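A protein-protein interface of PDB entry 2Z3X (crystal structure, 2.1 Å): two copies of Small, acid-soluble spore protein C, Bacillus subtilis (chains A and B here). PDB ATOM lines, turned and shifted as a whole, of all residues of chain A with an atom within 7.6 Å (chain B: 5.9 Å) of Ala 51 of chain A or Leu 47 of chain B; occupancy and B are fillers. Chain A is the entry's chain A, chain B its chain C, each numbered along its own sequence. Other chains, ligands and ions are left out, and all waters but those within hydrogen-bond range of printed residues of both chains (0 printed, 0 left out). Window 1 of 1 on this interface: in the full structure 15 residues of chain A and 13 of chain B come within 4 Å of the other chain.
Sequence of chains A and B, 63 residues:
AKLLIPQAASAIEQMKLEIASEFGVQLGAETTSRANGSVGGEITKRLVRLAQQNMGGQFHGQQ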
ATOM      1  N   LEU A   4      24.456  35.465  35.533  1.00  0.00           N
ATOM      2  CA  LEU A   4      25.631  34.812  34.974  1.00  0.00           C
ATOM      3  C   LEU A   4      26.392  35.844  34.139  1.00  0.00           C
ATOM      4  O   LEU A   4      27.614  35.949  34.225  1.00  0.00           O
ATOM      5  CB  LEU A   4      25.219  33.620  34.104  1.00  0.00           C
ATOM      6  CG  LEU A   4      24.978  32.286  34.826  1.00  0.00           C
ATOM      7  CD1 LEU A   4      24.033  32.482  35.991  1.00  0.00           C
ATOM      8  CD2 LEU A   4      24.422  31.266  33.845  1.00  0.00           C
ATOM      9  N   THR A  44      13.795  31.754  32.315  1.00  0.00           N
ATOM     10  CA  THR A  44      14.689  30.609  32.175  1.00  0.00           C
ATOM     11  C   THR A  44      14.304  29.734  30.983  1.00  0.00           C
ATOM     12  O   THR A  44      15.169  29.278  30.236  1.00  0.00           O
ATOM     13  CB  THR A  44      14.698  29.749  33.461  1.00  0.00           C
ATOM     14  OG1 THR A  44      15.277  30.502  34.531  1.00  0.00           O
ATOM     15  CG2 THR A  44      15.526  28.481  33.258  1.00  0.00           C
ATOM     16  N   LYS A  45      13.004  29.509  30.812  1.00  0.00           N
ATOM     17  CA  LYS A  45      12.515  28.688  29.719  1.00  0.00           C
ATOM     18  C   LYS A  45      12.903  29.303  28.377  1.00  0.00           C
ATOM     19  O   LYS A  45      13.523  28.647  27.540  1.00  0.00           O
ATOM     20  CB  LYS A  45      10.995  28.542  29.815  1.00  0.00           C
ATOM     21  CG  LYS A  45      10.384  27.669  28.740  1.00  0.00           C
ATOM     22  CD  LYS A  45       8.890  27.480  28.976  1.00  0.00           C
ATOM     23  CE  LYS A  45       8.277  26.591  27.906  1.00  0.00           C
ATOM     24  NZ  LYS A  45       6.812  26.399  28.115  1.00  0.00           N
ATOM     25  N   ARG A  46      12.545  30.566  28.176  1.00  0.00           N
ATOM     26  CA  ARG A  46      12.875  31.238  26.930  1.00  0.00           C
ATOM     27  C   ARG A  46      14.373  31.313  26.699  1.00  0.00           C
ATOM     28  O   ARG A  46      14.836  31.109  25.578  1.00  0.00           O
ATOM     29  CB  ARG A  46      12.275  32.637  26.897  1.00  0.00           C
ATOM     30  CG  ARG A  46      10.775  32.626  26.831  1.00  0.00           C
ATOM     31  CD  ARG A  46      10.246  34.019  26.637  1.00  0.00           C
ATOM     32  NE  ARG A  46       8.799  34.042  26.747  1.00  0.00           N
ATOM     33  CZ  ARG A  46       8.064  35.137  26.611  1.00  0.00           C
ATOM     34  NH1 ARG A  46       8.651  36.300  26.352  1.00  0.00           N
ATOM     35  NH2 ARG A  46       6.745  35.070  26.760  1.00  0.00           N
ATOM     36  N   LEU A  47      15.142  31.597  27.742  1.00  0.00           N
ATOM     37  CA  LEU A  47      16.587  31.662  27.563  1.00  0.00           C
ATOM     38  C   LEU A  47      17.149  30.309  27.140  1.00  0.00           C
ATOM     39  O   LEU A  47      17.984  30.229  26.237  1.00  0.00           O
ATOM     40  CB  LEU A  47      17.268  32.139  28.845  1.00  0.00           C
ATOM     41  CG  LEU A  47      17.022  33.619  29.126  1.00  0.00           C
ATOM     42  CD1 LEU A  47      17.663  34.011  30.441  1.00  0.00           C
ATOM     43  CD2 LEU A  47      17.598  34.449  27.974  1.00  0.00           C
ATOM     44  N   VAL A  48      16.687  29.249  27.793  1.00  0.00           N
ATOM     45  CA  VAL A  48      17.134  27.894  27.483  1.00  0.00           C
ATOM     46  C   VAL A  48      16.765  27.525  26.049  1.00  0.00           C
ATOM     47  O   VAL A  48      17.562  26.934  25.320  1.00  0.00           O
ATOM     48  CB  VAL A  48      16.483  26.857  28.437  1.00  0.00           C
ATOM     49  CG1 VAL A  48      16.752  25.447  27.939  1.00  0.00           C
ATOM     50  CG2 VAL A  48      17.029  27.026  29.847  1.00  0.00           C
ATOM     51  N   ARG A  49      15.545  27.869  25.657  1.00  0.00           N
ATOM     52  CA  ARG A  49      15.054  27.575  24.319  1.00  0.00           C
ATOM     53  C   ARG A  49      15.891  28.301  23.271  1.00  0.00           C
ATOM     54  O   ARG A  49      16.361  27.691  22.308  1.00  0.00           O
ATOM     55  CB  ARG A  49      13.585  27.990  24.211  1.00  0.00           C
ATOM     56  CG  ARG A  49      13.004  27.965  22.808  1.00  0.00           C
ATOM     57  CD  ARG A  49      11.520  28.322  22.850  1.00  0.00           C
ATOM     58  NE  ARG A  49      10.696  27.236  23.383  1.00  0.00           N
ATOM     59  CZ  ARG A  49       9.472  27.400  23.880  1.00  0.00           C
ATOM     60  NH1 ARG A  49       8.931  28.611  23.920  1.00  0.00           N
ATOM     61  NH2 ARG A  49       8.780  26.353  24.322  1.00  0.00           N
ATOM     62  N   LEU A  50      16.078  29.604  23.465  1.00  0.00           N
ATOM     63  CA  LEU A  50      16.866  30.405  22.538  1.00  0.00           C
ATOM     64  C   LEU A  50      18.275  29.838  22.419  1.00  0.00           C
ATOM     65  O   LEU A  50      18.860  29.839  21.339  1.00  0.00           O
ATOM     66  CB  LEU A  50      16.924  31.864  23.005  1.00  0.00           C
ATOM     67  CG  LEU A  50      15.577  32.597  23.043  1.00  0.00           C
ATOM     68  CD1 LEU A  50      15.749  33.969  23.681  1.00  0.00           C
ATOM     69  CD2 LEU A  50      15.022  32.720  21.630  1.00  0.00           C
ATOM     70  N   ALA A  51      18.817  29.345  23.526  1.00  0.00           N
ATOM     71  CA  ALA A  51      20.161  28.780  23.512  1.00  0.00           C
ATOM     72  C   ALA A  51      20.200  27.533  22.629  1.00  0.00           C
ATOM     73  O   ALA A  51      21.058  27.405  21.754  1.00  0.00           O
ATOM     74  CB  ALA A  51      20.606  28.441  24.928  1.00  0.00           C
ATOM     75  N   GLN A  52      19.264  26.618  22.860  1.00  0.00           N
ATOM     76  CA  GLN A  52      19.193  25.387  22.080  1.00  0.00           C
ATOM     77  C   GLN A  52      19.020  25.700  20.598  1.00  0.00           C
ATOM     78  O   GLN A  52      19.649  25.074  19.745  1.00  0.00           O
ATOM     79  CB  GLN A  52      18.026  24.523  22.561  1.00  0.00           C
ATOM     80  CG  GLN A  52      18.121  24.141  24.022  1.00  0.00           C
ATOM     81  CD  GLN A  52      16.958  23.296  24.484  1.00  0.00           C
ATOM     82  OE1 GLN A  52      16.823  23.012  25.674  1.00  0.00           O
ATOM     83  NE2 GLN A  52      16.109  22.883  23.547  1.00  0.00           N
ATOM     84  N   GLN A  53      18.161  26.666  20.298  1.00  0.00           N
ATOM     85  CA  GLN A  53      17.919  27.061  18.919  1.00  0.00           C
ATOM     86  C   GLN A  53      19.198  27.572  18.267  1.00  0.00           C
ATOM     87  O   GLN A  53      19.687  26.982  17.305  1.00  0.00           O
ATOM     88  CB  GLN A  53      16.840  28.138  18.860  1.00  0.00           C
ATOM     89  CG  GLN A  53      15.439  27.613  19.095  1.00  0.00           C
ATOM     90  CD  GLN A  53      14.400  28.715  19.067  1.00  0.00           C
ATOM     91  OE1 GLN A  53      13.199  28.449  18.992  1.00  0.00           O
ATOM     92  NE2 GLN A  53      14.857  29.961  19.133  1.00  0.00           N
ATOM     93  N   ASN A  54      19.737  28.668  18.795  1.00  0.00           N
ATOM     94  CA  ASN A  54      20.965  29.249  18.258  1.00  0.00           C
ATOM     95  C   ASN A  54      22.172  28.446  18.711  1.00  0.00           C
ATOM     96  O   ASN A  54      23.095  28.980  19.329  1.00  0.00           O
ATOM     97  CB  ASN A  54      21.110  30.704  18.712  1.00  0.00           C
ATOM     98  CG  ASN A  54      20.018  31.600  18.153  1.00  0.00           C
ATOM     99  OD1 ASN A  54      18.825  31.338  18.342  1.00  0.00           O
ATOM    100  ND2 ASN A  54      20.420  32.669  17.462  1.00  0.00           N
ATOM    101  N   MET A  55      22.154  27.156  18.394  1.00  0.00           N
ATOM    102  CA  MET A  55      23.232  26.247  18.757  1.00  0.00           C
ATOM    103  C   MET A  55      23.030  24.885  18.095  1.00  0.00           C
ATOM    104  O   MET A  55      23.953  24.327  17.498  1.00  0.00           O
ATOM    105  CB  MET A  55      23.281  26.075  20.275  1.00  0.00           C
ATOM    106  CG  MET A  55      24.301  25.062  20.755  1.00  0.00           C
ATOM    107  SD  MET A  55      24.099  24.727  22.509  1.00  0.00           S
ATOM    108  CE  MET A  55      22.653  23.652  22.464  1.00  0.00           C
ATOM    109  N   GLY A  56      21.816  24.353  18.211  1.00  0.00           N
ATOM    110  CA  GLY A  56      21.513  23.062  17.623  1.00  0.00           C
ATOM    111  C   GLY A  56      20.173  23.059  16.913  1.00  0.00           C
ATOM    112  O   GLY A  56      19.273  22.298  17.333  1.00  0.00           O
ATOM    113  N   ILE B  12      23.253  19.199  22.979  1.00  0.00           N
ATOM    114  CA  ILE B  12      23.339  18.920  24.410  1.00  0.00           C
ATOM    115  C   ILE B  12      24.066  17.603  24.662  1.00  0.00           C
ATOM    116  O   ILE B  12      24.865  17.492  25.591  1.00  0.00           O
ATOM    117  CB  ILE B  12      21.936  18.842  25.062  1.00  0.00           C
ATOM    118  CG1 ILE B  12      21.129  17.701  24.436  1.00  0.00           C
ATOM    119  CG2 ILE B  12      21.213  20.170  24.893  1.00  0.00           C
ATOM    120  CD1 ILE B  12      19.922  17.272  25.251  1.00  0.00           C
ATOM    121  N   MET B  15      27.616  18.320  24.895  1.00  0.00           N
ATOM    122  CA  MET B  15      27.903  19.080  26.106  1.00  0.00           C
ATOM    123  C   MET B  15      27.718  18.217  27.351  1.00  0.00           C
ATOM    124  O   MET B  15      28.407  18.401  28.360  1.00  0.00           O
ATOM    125  CB  MET B  15      26.996  20.312  26.180  1.00  0.00           C
ATOM    126  CG  MET B  15      27.309  21.240  27.344  1.00  0.00           C
ATOM    127  SD  MET B  15      26.315  22.753  27.329  1.00  0.00           S
ATOM    128  CE  MET B  15      27.500  23.923  26.655  1.00  0.00           C
ATOM    129  N   GLU B  42      24.767  21.785  35.279  1.00  0.00           N
ATOM    130  CA  GLU B  42      25.755  22.529  34.508  1.00  0.00           C
ATOM    131  C   GLU B  42      25.248  22.796  33.103  1.00  0.00           C
ATOM    132  O   GLU B  42      25.551  23.829  32.505  1.00  0.00           O
ATOM    133  CB  GLU B  42      27.062  21.754  34.432  1.00  0.00           C
ATOM    134  CG  GLU B  42      28.151  22.330  35.293  1.00  0.00           C
ATOM    135  CD  GLU B  42      28.631  23.672  34.800  1.00  0.00           C
ATOM    136  OE1 GLU B  42      29.001  23.763  33.612  1.00  0.00           O
ATOM    137  OE2 GLU B  42      28.653  24.631  35.598  1.00  0.00           O
ATOM    138  N   ILE B  43      24.474  21.856  32.579  1.00  0.00           N
ATOM    139  CA  ILE B  43      23.927  21.995  31.242  1.00  0.00           C
ATOM    140  C   ILE B  43      23.012  23.209  31.177  1.00  0.00           C
ATOM    141  O   ILE B  43      23.111  24.030  30.266  1.00  0.00           O
ATOM    142  CB  ILE B  43      23.130  20.739  30.835  1.00  0.00           C
ATOM    143  CG1 ILE B  43      24.075  19.540  30.728  1.00  0.00           C
ATOM    144  CG2 ILE B  43      22.419  20.976  29.515  1.00  0.00           C
ATOM    145  CD1 ILE B  43      23.373  18.231  30.414  1.00  0.00           C
ATOM    146  N   THR B  44      22.120  23.321  32.154  1.00  0.00           N
ATOM    147  CA  THR B  44      21.188  24.434  32.196  1.00  0.00           C
ATOM    148  C   THR B  44      21.955  25.731  32.416  1.00  0.00           C
ATOM    149  O   THR B  44      21.712  26.729  31.742  1.00  0.00           O
ATOM    150  CB  THR B  44      20.149  24.227  33.318  1.00  0.00           C
ATOM    151  OG1 THR B  44      19.309  23.119  32.975  1.00  0.00           O
ATOM    152  CG2 THR B  44      19.288  25.466  33.505  1.00  0.00           C
ATOM    153  N   LYS B  45      22.891  25.700  33.356  1.00  0.00           N
ATOM    154  CA  LYS B  45      23.702  26.866  33.666  1.00  0.00           C
ATOM    155  C   LYS B  45      24.404  27.407  32.420  1.00  0.00           C
ATOM    156  O   LYS B  45      24.500  28.620  32.224  1.00  0.00           O
ATOM    157  CB  LYS B  45      24.752  26.503  34.712  1.00  0.00           C
ATOM    158  CG  LYS B  45      25.617  27.669  35.130  1.00  0.00           C
ATOM    159  CD  LYS B  45      26.778  27.196  35.977  1.00  0.00           C
ATOM    160  CE  LYS B  45      27.641  28.352  36.434  1.00  0.00           C
ATOM    161  NZ  LYS B  45      28.806  27.877  37.233  1.00  0.00           N
ATOM    162  N   ARG B  46      24.899  26.507  31.579  1.00  0.00           N
ATOM    163  CA  ARG B  46      25.603  26.921  30.374  1.00  0.00           C
ATOM    164  C   ARG B  46      24.655  27.428  29.305  1.00  0.00           C
ATOM    165  O   ARG B  46      24.922  28.451  28.674  1.00  0.00           O
ATOM    166  CB  ARG B  46      26.456  25.771  29.836  1.00  0.00           C
ATOM    167  CG  ARG B  46      27.617  25.428  30.751  1.00  0.00           C
ATOM    168  CD  ARG B  46      28.449  24.279  30.212  1.00  0.00           C
ATOM    169  NE  ARG B  46      29.606  24.019  31.065  1.00  0.00           N
ATOM    170  CZ  ARG B  46      30.543  23.115  30.800  1.00  0.00           C
ATOM    171  NH1 ARG B  46      30.463  22.376  29.699  1.00  0.00           N
ATOM    172  NH2 ARG B  46      31.560  22.958  31.638  1.00  0.00           N
ATOM    173  N   LEU B  47      23.544  26.724  29.099  1.00  0.00           N
ATOM    174  CA  LEU B  47      22.577  27.165  28.106  1.00  0.00           C
ATOM    175  C   LEU B  47      22.127  28.584  28.449  1.00  0.00           C
ATOM    176  O   LEU B  47      22.014  29.437  27.570  1.00  0.00           O
ATOM    177  CB  LEU B  47      21.370  26.225  28.066  1.00  0.00           C
ATOM    178  CG  LEU B  47      21.609  24.857  27.416  1.00  0.00           C
ATOM    179  CD1 LEU B  47      20.352  24.012  27.502  1.00  0.00           C
ATOM    180  CD2 LEU B  47      22.010  25.048  25.959  1.00  0.00           C
ATOM    181  N   VAL B  48      21.887  28.841  29.732  1.00  0.00           N
ATOM    182  CA  VAL B  48      21.456  30.161  30.166  1.00  0.00           C
ATOM    183  C   VAL B  48      22.546  31.182  29.891  1.00  0.00           C
ATOM    184  O   VAL B  48      22.295  32.218  29.284  1.00  0.00           O
ATOM    185  CB  VAL B  48      21.119  30.178  31.682  1.00  0.00           C
ATOM    186  CG1 VAL B  48      20.772  31.597  32.137  1.00  0.00           C
ATOM    187  CG2 VAL B  48      19.948  29.243  31.963  1.00  0.00           C
ATOM    188  N   ARG B  49      23.759  30.883  30.344  1.00  0.00           N
ATOM    189  CA  ARG B  49      24.894  31.776  30.145  1.00  0.00           C
ATOM    190  C   ARG B  49      25.081  32.154  28.673  1.00  0.00           C
ATOM    191  O   ARG B  49      25.370  33.307  28.353  1.00  0.00           O
ATOM    192  CB  ARG B  49      26.166  31.122  30.689  1.00  0.00           C
ATOM    193  CG  ARG B  49      27.446  31.860  30.348  1.00  0.00           C
ATOM    194  CD  ARG B  49      28.507  31.656  31.423  1.00  0.00           C
ATOM    195  NE  ARG B  49      28.615  30.262  31.849  1.00  0.00           N
ATOM    196  CZ  ARG B  49      28.910  29.242  31.046  1.00  0.00           C
ATOM    197  NH1 ARG B  49      29.131  29.447  29.752  1.00  0.00           N
ATOM    198  NH2 ARG B  49      28.989  28.010  31.540  1.00  0.00           N
ATOM    199  N   LEU B  50      24.910  31.185  27.779  1.00  0.00           N
ATOM    200  CA  LEU B  50      25.060  31.445  26.357  1.00  0.00           C
ATOM    201  C   LEU B  50      23.938  32.366  25.881  1.00  0.00           C
ATOM    202  O   LEU B  50      24.183  33.354  25.189  1.00  0.00           O
ATOM    203  CB  LEU B  50      25.037  30.132  25.559  1.00  0.00           C
ATOM    204  CG  LEU B  50      26.163  29.121  25.836  1.00  0.00           C
ATOM    205  CD1 LEU B  50      25.915  27.846  25.043  1.00  0.00           C
ATOM    206  CD2 LEU B  50      27.520  29.720  25.471  1.00  0.00           C
ATOM    207  N   ALA B  51      22.708  32.046  26.260  1.00  0.00           N
ATOM    208  CA  ALA B  51      21.568  32.859  25.860  1.00  0.00           C
ATOM    209  C   ALA B  51      21.729  34.293  26.367  1.00  0.00           C
ATOM    210  O   ALA B  51      21.382  35.244  25.666  1.00  0.00           O
ATOM    211  CB  ALA B  51      20.272  32.248  26.388  1.00  0.00           C
ATOM    212  N   GLN B  52      22.252  34.452  27.581  1.00  0.00           N
ATOM    213  CA  GLN B  52      22.451  35.791  28.133  1.00  0.00           C
ATOM    214  C   GLN B  52      23.554  36.518  27.378  1.00  0.00           C
ATOM    215  O   GLN B  52      23.626  37.747  27.382  1.00  0.00           O
ATOM    216  CB  GLN B  52      22.807  35.727  29.622  1.00  0.00           C
ATOM    217  CG  GLN B  52      21.627  35.438  30.532  1.00  0.00           C
ATOM    218  CD  GLN B  52      21.983  35.556  32.004  1.00  0.00           C
ATOM    219  OE1 GLN B  52      21.133  35.371  32.880  1.00  0.00           O
ATOM    220  NE2 GLN B  52      23.241  35.865  32.285  1.00  0.00           N
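The side-chain amide nitrogen (NE2) of Gln 52 of chain B sits close to the backbone NH (N) of Leu 4 of chain A, at 3.5 Å.
OE2 of Glu 42 of chain B lies within salt-bridge range of NZ of Lys 45 of chain B (3.6 Å).
Leu 4 of chain A touches Lys 45 of chain B (CD2 to O, 3.1 Å). N of Arg 49 of chain B touches CD2 of Leu 4 of chain A, at 3.6 Å. CB of Ala 51 of chain B touches O of Leu 47 of chain A (3.1 Å). CG1 of Val 48 of chain A touches CD1 of Leu 47 of chain B (3.9 Å). Leu 47 of chain B touches Ala 51 of chain A (O to CB, 3.2 Å). Leu 47 of chain B touches Met 55 of chain A (CD2 to CE, 3.8 Å).
Of the printed residues of chain B, Leu 4 of chain A touches Lys 45, Arg 49 and Gln 52. Printed residues of chain B within 4 Å of Val 48 of chain A: Leu 47 (3.9 Å). Printed residues of chain B within 4 Å of Ala 51 of chain A: Leu 47. Ile 12 of chain B touches none of the printed residues of chain A. Leu 47 of chain B touches just these residues of chain A: Val 48, Ala 51 and Met 55. Val 48 of chain B touches none of the printed residues of chain A. Of the printed residues of chain A, Arg 49 of chain B touches Leu 4. The nearest residue of chain B that does not touch Ala 51 of chain A is Ala 51 of chain B (4.1 Å).
Among the printed residues, no Asp or Glu carboxylate lies within 4 Å of a Lys or Arg side-chain nitrogen of the other chain.
Leu 47 of chain A touches Ala 51 of chain B, and with the chains exchanged Ala 51 of chain A touches Leu 47 of chain B. Val 48 of chain A touches Leu 47 of chain B, but with the chains exchanged Leu 47 of chain A does not touch Val 48 of chain B (4.3 Å). Of the 7 pairs that touch across the chains among the printed residues, 2 have their exchanged pair printed and touching as well.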
